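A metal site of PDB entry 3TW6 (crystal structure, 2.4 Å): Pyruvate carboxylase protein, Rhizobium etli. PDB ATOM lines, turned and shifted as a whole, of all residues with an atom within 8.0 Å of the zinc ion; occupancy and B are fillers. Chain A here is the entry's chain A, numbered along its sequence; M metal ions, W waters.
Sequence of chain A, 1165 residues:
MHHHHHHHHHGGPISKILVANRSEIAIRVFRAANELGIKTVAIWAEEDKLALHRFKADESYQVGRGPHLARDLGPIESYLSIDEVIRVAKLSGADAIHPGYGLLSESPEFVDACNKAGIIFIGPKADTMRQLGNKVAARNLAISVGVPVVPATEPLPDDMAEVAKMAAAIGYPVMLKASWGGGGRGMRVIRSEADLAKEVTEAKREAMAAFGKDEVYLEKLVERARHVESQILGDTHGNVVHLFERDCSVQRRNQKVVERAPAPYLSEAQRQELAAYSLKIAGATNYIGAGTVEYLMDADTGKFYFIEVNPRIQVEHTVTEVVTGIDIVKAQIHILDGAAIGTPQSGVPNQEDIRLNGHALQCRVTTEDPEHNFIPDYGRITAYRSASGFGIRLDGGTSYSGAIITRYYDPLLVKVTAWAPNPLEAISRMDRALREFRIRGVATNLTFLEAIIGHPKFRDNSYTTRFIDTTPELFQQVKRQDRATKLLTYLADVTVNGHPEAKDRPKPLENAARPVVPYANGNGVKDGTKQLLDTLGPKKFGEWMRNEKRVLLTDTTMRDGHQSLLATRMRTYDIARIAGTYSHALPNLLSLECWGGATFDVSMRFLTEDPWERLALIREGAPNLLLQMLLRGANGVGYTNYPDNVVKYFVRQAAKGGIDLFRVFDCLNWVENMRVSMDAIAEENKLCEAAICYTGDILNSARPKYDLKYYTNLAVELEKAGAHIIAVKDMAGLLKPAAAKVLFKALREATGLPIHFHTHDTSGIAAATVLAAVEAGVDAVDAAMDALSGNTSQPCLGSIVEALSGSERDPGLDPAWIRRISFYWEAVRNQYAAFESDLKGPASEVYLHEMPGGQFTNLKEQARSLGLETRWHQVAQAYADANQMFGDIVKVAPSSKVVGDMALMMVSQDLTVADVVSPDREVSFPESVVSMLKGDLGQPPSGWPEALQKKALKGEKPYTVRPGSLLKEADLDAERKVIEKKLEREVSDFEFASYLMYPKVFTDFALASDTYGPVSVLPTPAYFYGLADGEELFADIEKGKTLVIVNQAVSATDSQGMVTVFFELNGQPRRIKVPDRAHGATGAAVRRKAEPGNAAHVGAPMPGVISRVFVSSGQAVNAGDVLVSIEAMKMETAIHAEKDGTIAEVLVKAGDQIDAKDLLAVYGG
The side-chain carboxylate (OD1) of Asp 560 is in salt-bridge range of the guanidinium group (NH2) of Arg 559 (3.3 Å).
N of Asp 560 lies within hydrogen-bond range of OE1 of Glu 593 (3.2 Å).
A ring nitrogen (NE2) of His 758 lies close to the side-chain amide nitrogen (NE2) of Gln 794 (3.4 Å).
A ring nitrogen (ND1) of His 760 lies close to the side-chain amide nitrogen (NE2) of Gln 794.
ND1 of His 760 is in hydrogen-bond range of O of Thr 792 (2.6 Å).
NH1 of Arg 559 lies close to OQ2 of KCX 729 (2.8 Å).
The side-chain amide nitrogen (NE2) of Gln 794 is in hydrogen-bond range of the backbone carbonyl oxygen (O) of Thr 759 (3.0 Å).
The side-chain amide oxygen of Gln 794 sits at hydrogen-bond distance from the side-chain hydroxyl of Thr 556 (2.9 Å).
NH1 of Arg 559 touches the zinc ion, at 3.98 Å.
NE2 of Gln 794 touches the zinc ion, at 3.8 Å.
Six residues have an atom within 4 Å of the zinc ion: Arg 559, Asp 560, KCX 729, His 758, His 760 and Gln 794.
The nearest printed residue that does not touch the zinc ion is Met 731 (4.9 Å).
The zinc ion is bound by OD2 of Asp 560 (2.1 Å), NE2 of His 758 (2.2 Å), NE2 of His 760 (2.3 Å), OQ2 of KCX 729 (2.3 Å), water W1 (2.4 Å) and OQ1 of KCX 729 (2.4 Å).
The zinc ion has six donor atoms within binding distance.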
ATOM      1  N   THR A 556      -0.177 -17.258 -13.231  1.00  0.00           N
ATOM      2  CA  THR A 556       0.697 -16.173 -12.943  1.00  0.00           C
ATOM      3  C   THR A 556       1.768 -16.561 -11.879  1.00  0.00           C
ATOM      4  O   THR A 556       2.516 -15.695 -11.410  1.00  0.00           O
ATOM      5  CB  THR A 556      -0.106 -15.007 -12.308  1.00  0.00           C
ATOM      6  OG1 THR A 556      -0.704 -15.529 -11.126  1.00  0.00           O
ATOM      7  CG2 THR A 556      -1.164 -14.456 -13.215  1.00  0.00           C
ATOM      8  N   ARG A 559       5.353 -15.083 -12.092  1.00  0.00           N
ATOM      9  CA  ARG A 559       5.613 -13.593 -11.959  1.00  0.00           C
ATOM     10  C   ARG A 559       4.847 -13.000 -10.744  1.00  0.00           C
ATOM     11  O   ARG A 559       5.441 -12.844  -9.659  1.00  0.00           O
ATOM     12  CB  ARG A 559       5.352 -12.847 -13.295  1.00  0.00           C
ATOM     13  CG  ARG A 559       5.881 -11.398 -13.470  1.00  0.00           C
ATOM     14  CD  ARG A 559       5.221 -10.339 -12.563  1.00  0.00           C
ATOM     15  NE  ARG A 559       3.789 -10.115 -12.815  1.00  0.00           N
ATOM     16  CZ  ARG A 559       3.063  -9.093 -12.333  1.00  0.00           C
ATOM     17  NH1 ARG A 559       1.745  -9.053 -12.619  1.00  0.00           N
ATOM     18  NH2 ARG A 559       3.614  -8.157 -11.516  1.00  0.00           N
ATOM     19  N   ASP A 560       3.528 -12.746 -10.900  1.00  0.00           N
ATOM     20  CA  ASP A 560       2.713 -12.065  -9.877  1.00  0.00           C
ATOM     21  C   ASP A 560       2.601 -12.862  -8.553  1.00  0.00           C
ATOM     22  O   ASP A 560       2.719 -12.291  -7.452  1.00  0.00           O
ATOM     23  CB  ASP A 560       1.363 -11.633 -10.463  1.00  0.00           C
ATOM     24  CG  ASP A 560       0.814 -10.310  -9.874  1.00  0.00           C
ATOM     25  OD1 ASP A 560       1.538  -9.467  -9.299  1.00  0.00           O
ATOM     26  OD2 ASP A 560      -0.402 -10.071 -10.036  1.00  0.00           O
ATOM     27  N   GLY A 561       2.478 -14.190  -8.636  1.00  0.00           N
ATOM     28  CA  GLY A 561       2.415 -15.042  -7.394  1.00  0.00           C
ATOM     29  C   GLY A 561       3.634 -14.792  -6.512  1.00  0.00           C
ATOM     30  O   GLY A 561       3.504 -14.432  -5.303  1.00  0.00           O
ATOM     31  N   GLN A 563       5.967 -12.357  -6.987  1.00  0.00           N
ATOM     32  CA  GLN A 563       6.040 -10.914  -6.721  1.00  0.00           C
ATOM     33  C   GLN A 563       5.199 -10.506  -5.462  1.00  0.00           C
ATOM     34  O   GLN A 563       5.631  -9.701  -4.618  1.00  0.00           O
ATOM     35  CB  GLN A 563       5.642 -10.044  -7.944  1.00  0.00           C
ATOM     36  CG  GLN A 563       5.653  -8.536  -7.634  1.00  0.00           C
ATOM     37  CD  GLN A 563       5.765  -7.666  -8.901  1.00  0.00           C
ATOM     38  OE1 GLN A 563       6.252  -8.089  -9.984  1.00  0.00           O
ATOM     39  NE2 GLN A 563       5.358  -6.399  -8.770  1.00  0.00           N
ATOM     40  N   SER A 564       4.018 -11.091  -5.306  1.00  0.00           N
ATOM     41  CA  SER A 564       3.132 -10.676  -4.262  1.00  0.00           C
ATOM     42  C   SER A 564       3.518 -11.350  -3.003  1.00  0.00           C
ATOM     43  O   SER A 564       3.282 -10.819  -1.925  1.00  0.00           O
ATOM     44  CB  SER A 564       1.708 -11.025  -4.594  1.00  0.00           C
ATOM     45  OG  SER A 564       1.329 -10.341  -5.779  1.00  0.00           O
ATOM     46  N   GLU A 593       2.092 -16.039 -17.316  1.00  0.00           N
ATOM     47  CA  GLU A 593       2.611 -14.696 -17.036  1.00  0.00           C
ATOM     48  C   GLU A 593       3.944 -14.972 -16.278  1.00  0.00           C
ATOM     49  O   GLU A 593       3.931 -15.642 -15.229  1.00  0.00           O
ATOM     50  CB  GLU A 593       1.628 -13.797 -16.214  1.00  0.00           C
ATOM     51  CG  GLU A 593       2.233 -12.374 -15.996  1.00  0.00           C
ATOM     52  CD  GLU A 593       1.717 -11.636 -14.733  1.00  0.00           C
ATOM     53  OE1 GLU A 593       1.992 -12.120 -13.593  1.00  0.00           O
ATOM     54  OE2 GLU A 593       1.068 -10.548 -14.865  1.00  0.00           O
ATOM     55  N   LEU A 630       3.962  -8.358 -17.856  1.00  0.00           N
ATOM     56  CA  LEU A 630       3.280  -7.136 -17.531  1.00  0.00           C
ATOM     57  C   LEU A 630       4.198  -6.028 -17.997  1.00  0.00           C
ATOM     58  O   LEU A 630       5.358  -6.038 -17.662  1.00  0.00           O
ATOM     59  CB  LEU A 630       3.072  -6.999 -16.040  1.00  0.00           C
ATOM     60  CG  LEU A 630       2.199  -5.814 -15.613  1.00  0.00           C
ATOM     61  CD1 LEU A 630       0.703  -5.962 -15.964  1.00  0.00           C
ATOM     62  CD2 LEU A 630       2.373  -5.524 -14.132  1.00  0.00           C
ATOM     63  N   ARG A 663       0.812  -7.393 -21.602  1.00  0.00           N
ATOM     64  CA  ARG A 663      -0.332  -6.794 -20.920  1.00  0.00           C
ATOM     65  C   ARG A 663       0.136  -5.395 -20.508  1.00  0.00           C
ATOM     66  O   ARG A 663       1.061  -5.262 -19.673  1.00  0.00           O
ATOM     67  CB  ARG A 663      -0.707  -7.546 -19.668  1.00  0.00           C
ATOM     68  CG  ARG A 663      -1.698  -6.703 -18.777  1.00  0.00           C
ATOM     69  CD  ARG A 663      -2.250  -7.491 -17.584  1.00  0.00           C
ATOM     70  NE  ARG A 663      -2.976  -8.719 -17.968  1.00  0.00           N
ATOM     71  CZ  ARG A 663      -3.129  -9.814 -17.185  1.00  0.00           C
ATOM     72  NH1 ARG A 663      -2.543  -9.912 -15.981  1.00  0.00           N
ATOM     73  NH2 ARG A 663      -3.869 -10.825 -17.610  1.00  0.00           N
ATOM     74  N   KCX A 729      -7.569  -4.988 -14.930  1.00  0.00           N
ATOM     75  CA  KCX A 729      -6.561  -5.290 -13.924  1.00  0.00           C
ATOM     76  CB  KCX A 729      -5.273  -4.666 -14.410  1.00  0.00           C
ATOM     77  CG  KCX A 729      -4.055  -4.869 -13.484  1.00  0.00           C
ATOM     78  CD  KCX A 729      -2.864  -4.065 -14.053  1.00  0.00           C
ATOM     79  CE  KCX A 729      -1.720  -3.891 -13.043  1.00  0.00           C
ATOM     80  NZ  KCX A 729      -1.045  -5.157 -12.951  1.00  0.00           N
ATOM     81  C   KCX A 729      -7.018  -4.697 -12.605  1.00  0.00           C
ATOM     82  O   KCX A 729      -6.957  -3.477 -12.381  1.00  0.00           O
ATOM     83  CX  KCX A 729      -1.108  -6.116 -12.035  1.00  0.00           C
ATOM     84  OQ1 KCX A 729      -1.804  -6.010 -11.090  1.00  0.00           O
ATOM     85  OQ2 KCX A 729      -0.403  -7.244 -12.169  1.00  0.00           O
ATOM     86  N   ASP A 730      -7.443  -5.578 -11.739  1.00  0.00           N
ATOM     87  CA  ASP A 730      -7.927  -5.279 -10.426  1.00  0.00           C
ATOM     88  C   ASP A 730      -6.718  -5.571  -9.499  1.00  0.00           C
ATOM     89  O   ASP A 730      -6.635  -6.597  -8.790  1.00  0.00           O
ATOM     90  CB  ASP A 730      -9.125  -6.216 -10.195  1.00  0.00           C
ATOM     91  CG  ASP A 730      -9.767  -6.040  -8.839  1.00  0.00           C
ATOM     92  OD1 ASP A 730      -9.622  -4.960  -8.260  1.00  0.00           O
ATOM     93  OD2 ASP A 730     -10.361  -7.028  -8.300  1.00  0.00           O
ATOM     94  N   MET A 731      -5.793  -4.634  -9.512  1.00  0.00           N
ATOM     95  CA  MET A 731      -4.521  -4.787  -8.809  1.00  0.00           C
ATOM     96  C   MET A 731      -4.721  -4.857  -7.285  1.00  0.00           C
ATOM     97  O   MET A 731      -3.883  -5.446  -6.594  1.00  0.00           O
ATOM     98  CB  MET A 731      -3.535  -3.608  -9.174  1.00  0.00           C
ATOM     99  CG  MET A 731      -4.003  -2.219  -8.729  1.00  0.00           C
ATOM    100  SD  MET A 731      -5.077  -1.603 -10.026  1.00  0.00           S
ATOM    101  CE  MET A 731      -5.904  -0.204  -9.257  1.00  0.00           C
ATOM    102  N   ALA A 732      -5.799  -4.284  -6.758  1.00  0.00           N
ATOM    103  CA  ALA A 732      -6.013  -4.367  -5.296  1.00  0.00           C
ATOM    104  C   ALA A 732      -7.027  -5.430  -4.877  1.00  0.00           C
ATOM    105  O   ALA A 732      -7.345  -5.554  -3.703  1.00  0.00           O
ATOM    106  CB  ALA A 732      -6.345  -3.003  -4.659  1.00  0.00           C
ATOM    107  N   GLY A 733      -7.598  -6.158  -5.833  1.00  0.00           N
ATOM    108  CA  GLY A 733      -8.642  -7.173  -5.433  1.00  0.00           C
ATOM    109  C   GLY A 733      -9.976  -6.565  -4.994  1.00  0.00           C
ATOM    110  O   GLY A 733     -10.658  -7.158  -4.122  1.00  0.00           O
ATOM    111  N   HIS A 758      -7.793 -10.041 -14.465  1.00  0.00           N
ATOM    112  CA  HIS A 758      -6.759 -10.328 -13.482  1.00  0.00           C
ATOM    113  C   HIS A 758      -7.096  -9.698 -12.170  1.00  0.00           C
ATOM    114  O   HIS A 758      -7.266  -8.442 -12.061  1.00  0.00           O
ATOM    115  CB  HIS A 758      -5.467  -9.682 -13.993  1.00  0.00           C
ATOM    116  CG  HIS A 758      -4.344  -9.681 -12.998  1.00  0.00           C
ATOM    117  ND1 HIS A 758      -3.406 -10.674 -12.945  1.00  0.00           N
ATOM    118  CD2 HIS A 758      -4.004  -8.757 -12.017  1.00  0.00           C
ATOM    119  CE1 HIS A 758      -2.510 -10.366 -11.956  1.00  0.00           C
ATOM    120  NE2 HIS A 758      -2.872  -9.220 -11.411  1.00  0.00           N
ATOM    121  N   THR A 759      -7.080 -10.466 -11.109  1.00  0.00           N
ATOM    122  CA  THR A 759      -7.362  -9.882  -9.781  1.00  0.00           C
ATOM    123  C   THR A 759      -6.449 -10.460  -8.645  1.00  0.00           C
ATOM    124  O   THR A 759      -5.637 -11.398  -8.862  1.00  0.00           O
ATOM    125  CB  THR A 759      -8.880 -10.173  -9.419  1.00  0.00           C
ATOM    126  OG1 THR A 759      -9.268  -9.391  -8.264  1.00  0.00           O
ATOM    127  CG2 THR A 759      -9.114 -11.715  -9.178  1.00  0.00           C
ATOM    128  N   HIS A 760      -6.625  -9.965  -7.428  1.00  0.00           N
ATOM    129  CA  HIS A 760      -5.850 -10.448  -6.313  1.00  0.00           C
ATOM    130  C   HIS A 760      -6.766 -10.807  -5.165  1.00  0.00           C
ATOM    131  O   HIS A 760      -7.868 -10.258  -5.051  1.00  0.00           O
ATOM    132  CB  HIS A 760      -4.938  -9.342  -5.831  1.00  0.00           C
ATOM    133  CG  HIS A 760      -3.741  -9.095  -6.693  1.00  0.00           C
ATOM    134  ND1 HIS A 760      -2.483  -9.565  -6.353  1.00  0.00           N
ATOM    135  CD2 HIS A 760      -3.588  -8.360  -7.870  1.00  0.00           C
ATOM    136  CE1 HIS A 760      -1.588  -9.102  -7.223  1.00  0.00           C
ATOM    137  NE2 HIS A 760      -2.249  -8.418  -8.171  1.00  0.00           N
ATOM    138  N   ASP A 782      -6.942 -14.879 -14.847  1.00  0.00           N
ATOM    139  CA  ASP A 782      -5.636 -15.234 -14.228  1.00  0.00           C
ATOM    140  C   ASP A 782      -5.842 -16.003 -12.914  1.00  0.00           C
ATOM    141  O   ASP A 782      -6.742 -15.666 -12.119  1.00  0.00           O
ATOM    142  CB  ASP A 782      -4.817 -13.994 -13.848  1.00  0.00           C
ATOM    143  CG  ASP A 782      -4.262 -13.247 -15.076  1.00  0.00           C
ATOM    144  OD1 ASP A 782      -4.755 -13.477 -16.196  1.00  0.00           O
ATOM    145  OD2 ASP A 782      -3.300 -12.389 -14.935  1.00  0.00           O
ATOM    146  N   THR A 792      -2.325 -11.733  -0.762  1.00  0.00           N
ATOM    147  CA  THR A 792      -2.116 -10.682  -1.746  1.00  0.00           C
ATOM    148  C   THR A 792      -1.778 -11.192  -3.146  1.00  0.00           C
ATOM    149  O   THR A 792      -1.465 -10.367  -4.091  1.00  0.00           O
ATOM    150  CB  THR A 792      -0.942  -9.820  -1.294  1.00  0.00           C
ATOM    151  OG1 THR A 792       0.166 -10.725  -1.029  1.00  0.00           O
ATOM    152  CG2 THR A 792      -1.283  -8.997  -0.067  1.00  0.00           C
ATOM    153  N   SER A 793      -1.795 -12.505  -3.341  1.00  0.00           N
ATOM    154  CA  SER A 793      -1.576 -13.096  -4.681  1.00  0.00           C
ATOM    155  C   SER A 793      -2.881 -13.323  -5.478  1.00  0.00           C
ATOM    156  O   SER A 793      -3.956 -12.823  -5.056  1.00  0.00           O
ATOM    157  CB  SER A 793      -0.764 -14.407  -4.511  1.00  0.00           C
ATOM    158  OG  SER A 793      -0.465 -15.046  -5.796  1.00  0.00           O
ATOM    159  N   GLN A 794      -2.856 -14.071  -6.605  1.00  0.00           N
ATOM    160  CA  GLN A 794      -4.031 -14.346  -7.312  1.00  0.00           C
ATOM    161  C   GLN A 794      -4.792 -15.432  -6.535  1.00  0.00           C
ATOM    162  O   GLN A 794      -4.264 -16.043  -5.579  1.00  0.00           O
ATOM    163  CB  GLN A 794      -3.707 -14.859  -8.729  1.00  0.00           C
ATOM    164  CG  GLN A 794      -3.491 -13.738  -9.778  1.00  0.00           C
ATOM    165  CD  GLN A 794      -2.339 -12.865  -9.369  1.00  0.00           C
ATOM    166  OE1 GLN A 794      -1.163 -13.343  -9.328  1.00  0.00           O
ATOM    167  NE2 GLN A 794      -2.628 -11.585  -9.026  1.00  0.00           N
ATOM    168  N   PRO A 852      -2.737  -2.027  -3.316  1.00  0.00           N
ATOM    169  CA  PRO A 852      -2.662  -3.160  -4.242  1.00  0.00           C
ATOM    170  C   PRO A 852      -1.902  -4.331  -3.665  1.00  0.00           C
ATOM    171  O   PRO A 852      -0.862  -4.137  -3.082  1.00  0.00           O
ATOM    172  CB  PRO A 852      -1.893  -2.598  -5.460  1.00  0.00           C
ATOM    173  CG  PRO A 852      -1.346  -1.266  -5.084  1.00  0.00           C
ATOM    174  CD  PRO A 852      -2.050  -0.810  -3.818  1.00  0.00           C
ATOM    175  N   GLY A 853      -2.389  -5.559  -3.876  1.00  0.00           N
ATOM    176  CA  GLY A 853      -1.725  -6.748  -3.356  1.00  0.00           C
ATOM    177  C   GLY A 853      -0.209  -6.801  -3.541  1.00  0.00           C
ATOM    178  O   GLY A 853       0.570  -7.070  -2.609  1.00  0.00           O
ATOM    179  N   GLY A 854       0.219  -6.517  -4.765  1.00  0.00           N
ATOM    180  CA  GLY A 854       1.619  -6.295  -5.087  1.00  0.00           C
ATOM    181  C   GLY A 854       2.392  -5.243  -4.305  1.00  0.00           C
ATOM    182  O   GLY A 854       3.498  -4.941  -4.698  1.00  0.00           O
ATOM    183  N   VAL A 892      -1.513   2.151  -8.373  1.00  0.00           N
ATOM    184  CA  VAL A 892      -0.852   0.917  -8.814  1.00  0.00           C
ATOM    185  C   VAL A 892       0.609   1.291  -9.115  1.00  0.00           C
ATOM    186  O   VAL A 892       0.859   2.388  -9.602  1.00  0.00           O
ATOM    187  CB  VAL A 892      -1.550   0.418 -10.112  1.00  0.00           C
ATOM    188  CG1 VAL A 892      -1.451   1.466 -11.233  1.00  0.00           C
ATOM    189  CG2 VAL A 892      -1.023  -0.956 -10.604  1.00  0.00           C
HETATM  190 ZN    ZN M   1      -1.306  -8.180 -10.220  1.00  0.00          ZN
HETATM  191  O   HOH W   1       0.500  -7.317  -8.960  1.00  0.00           O
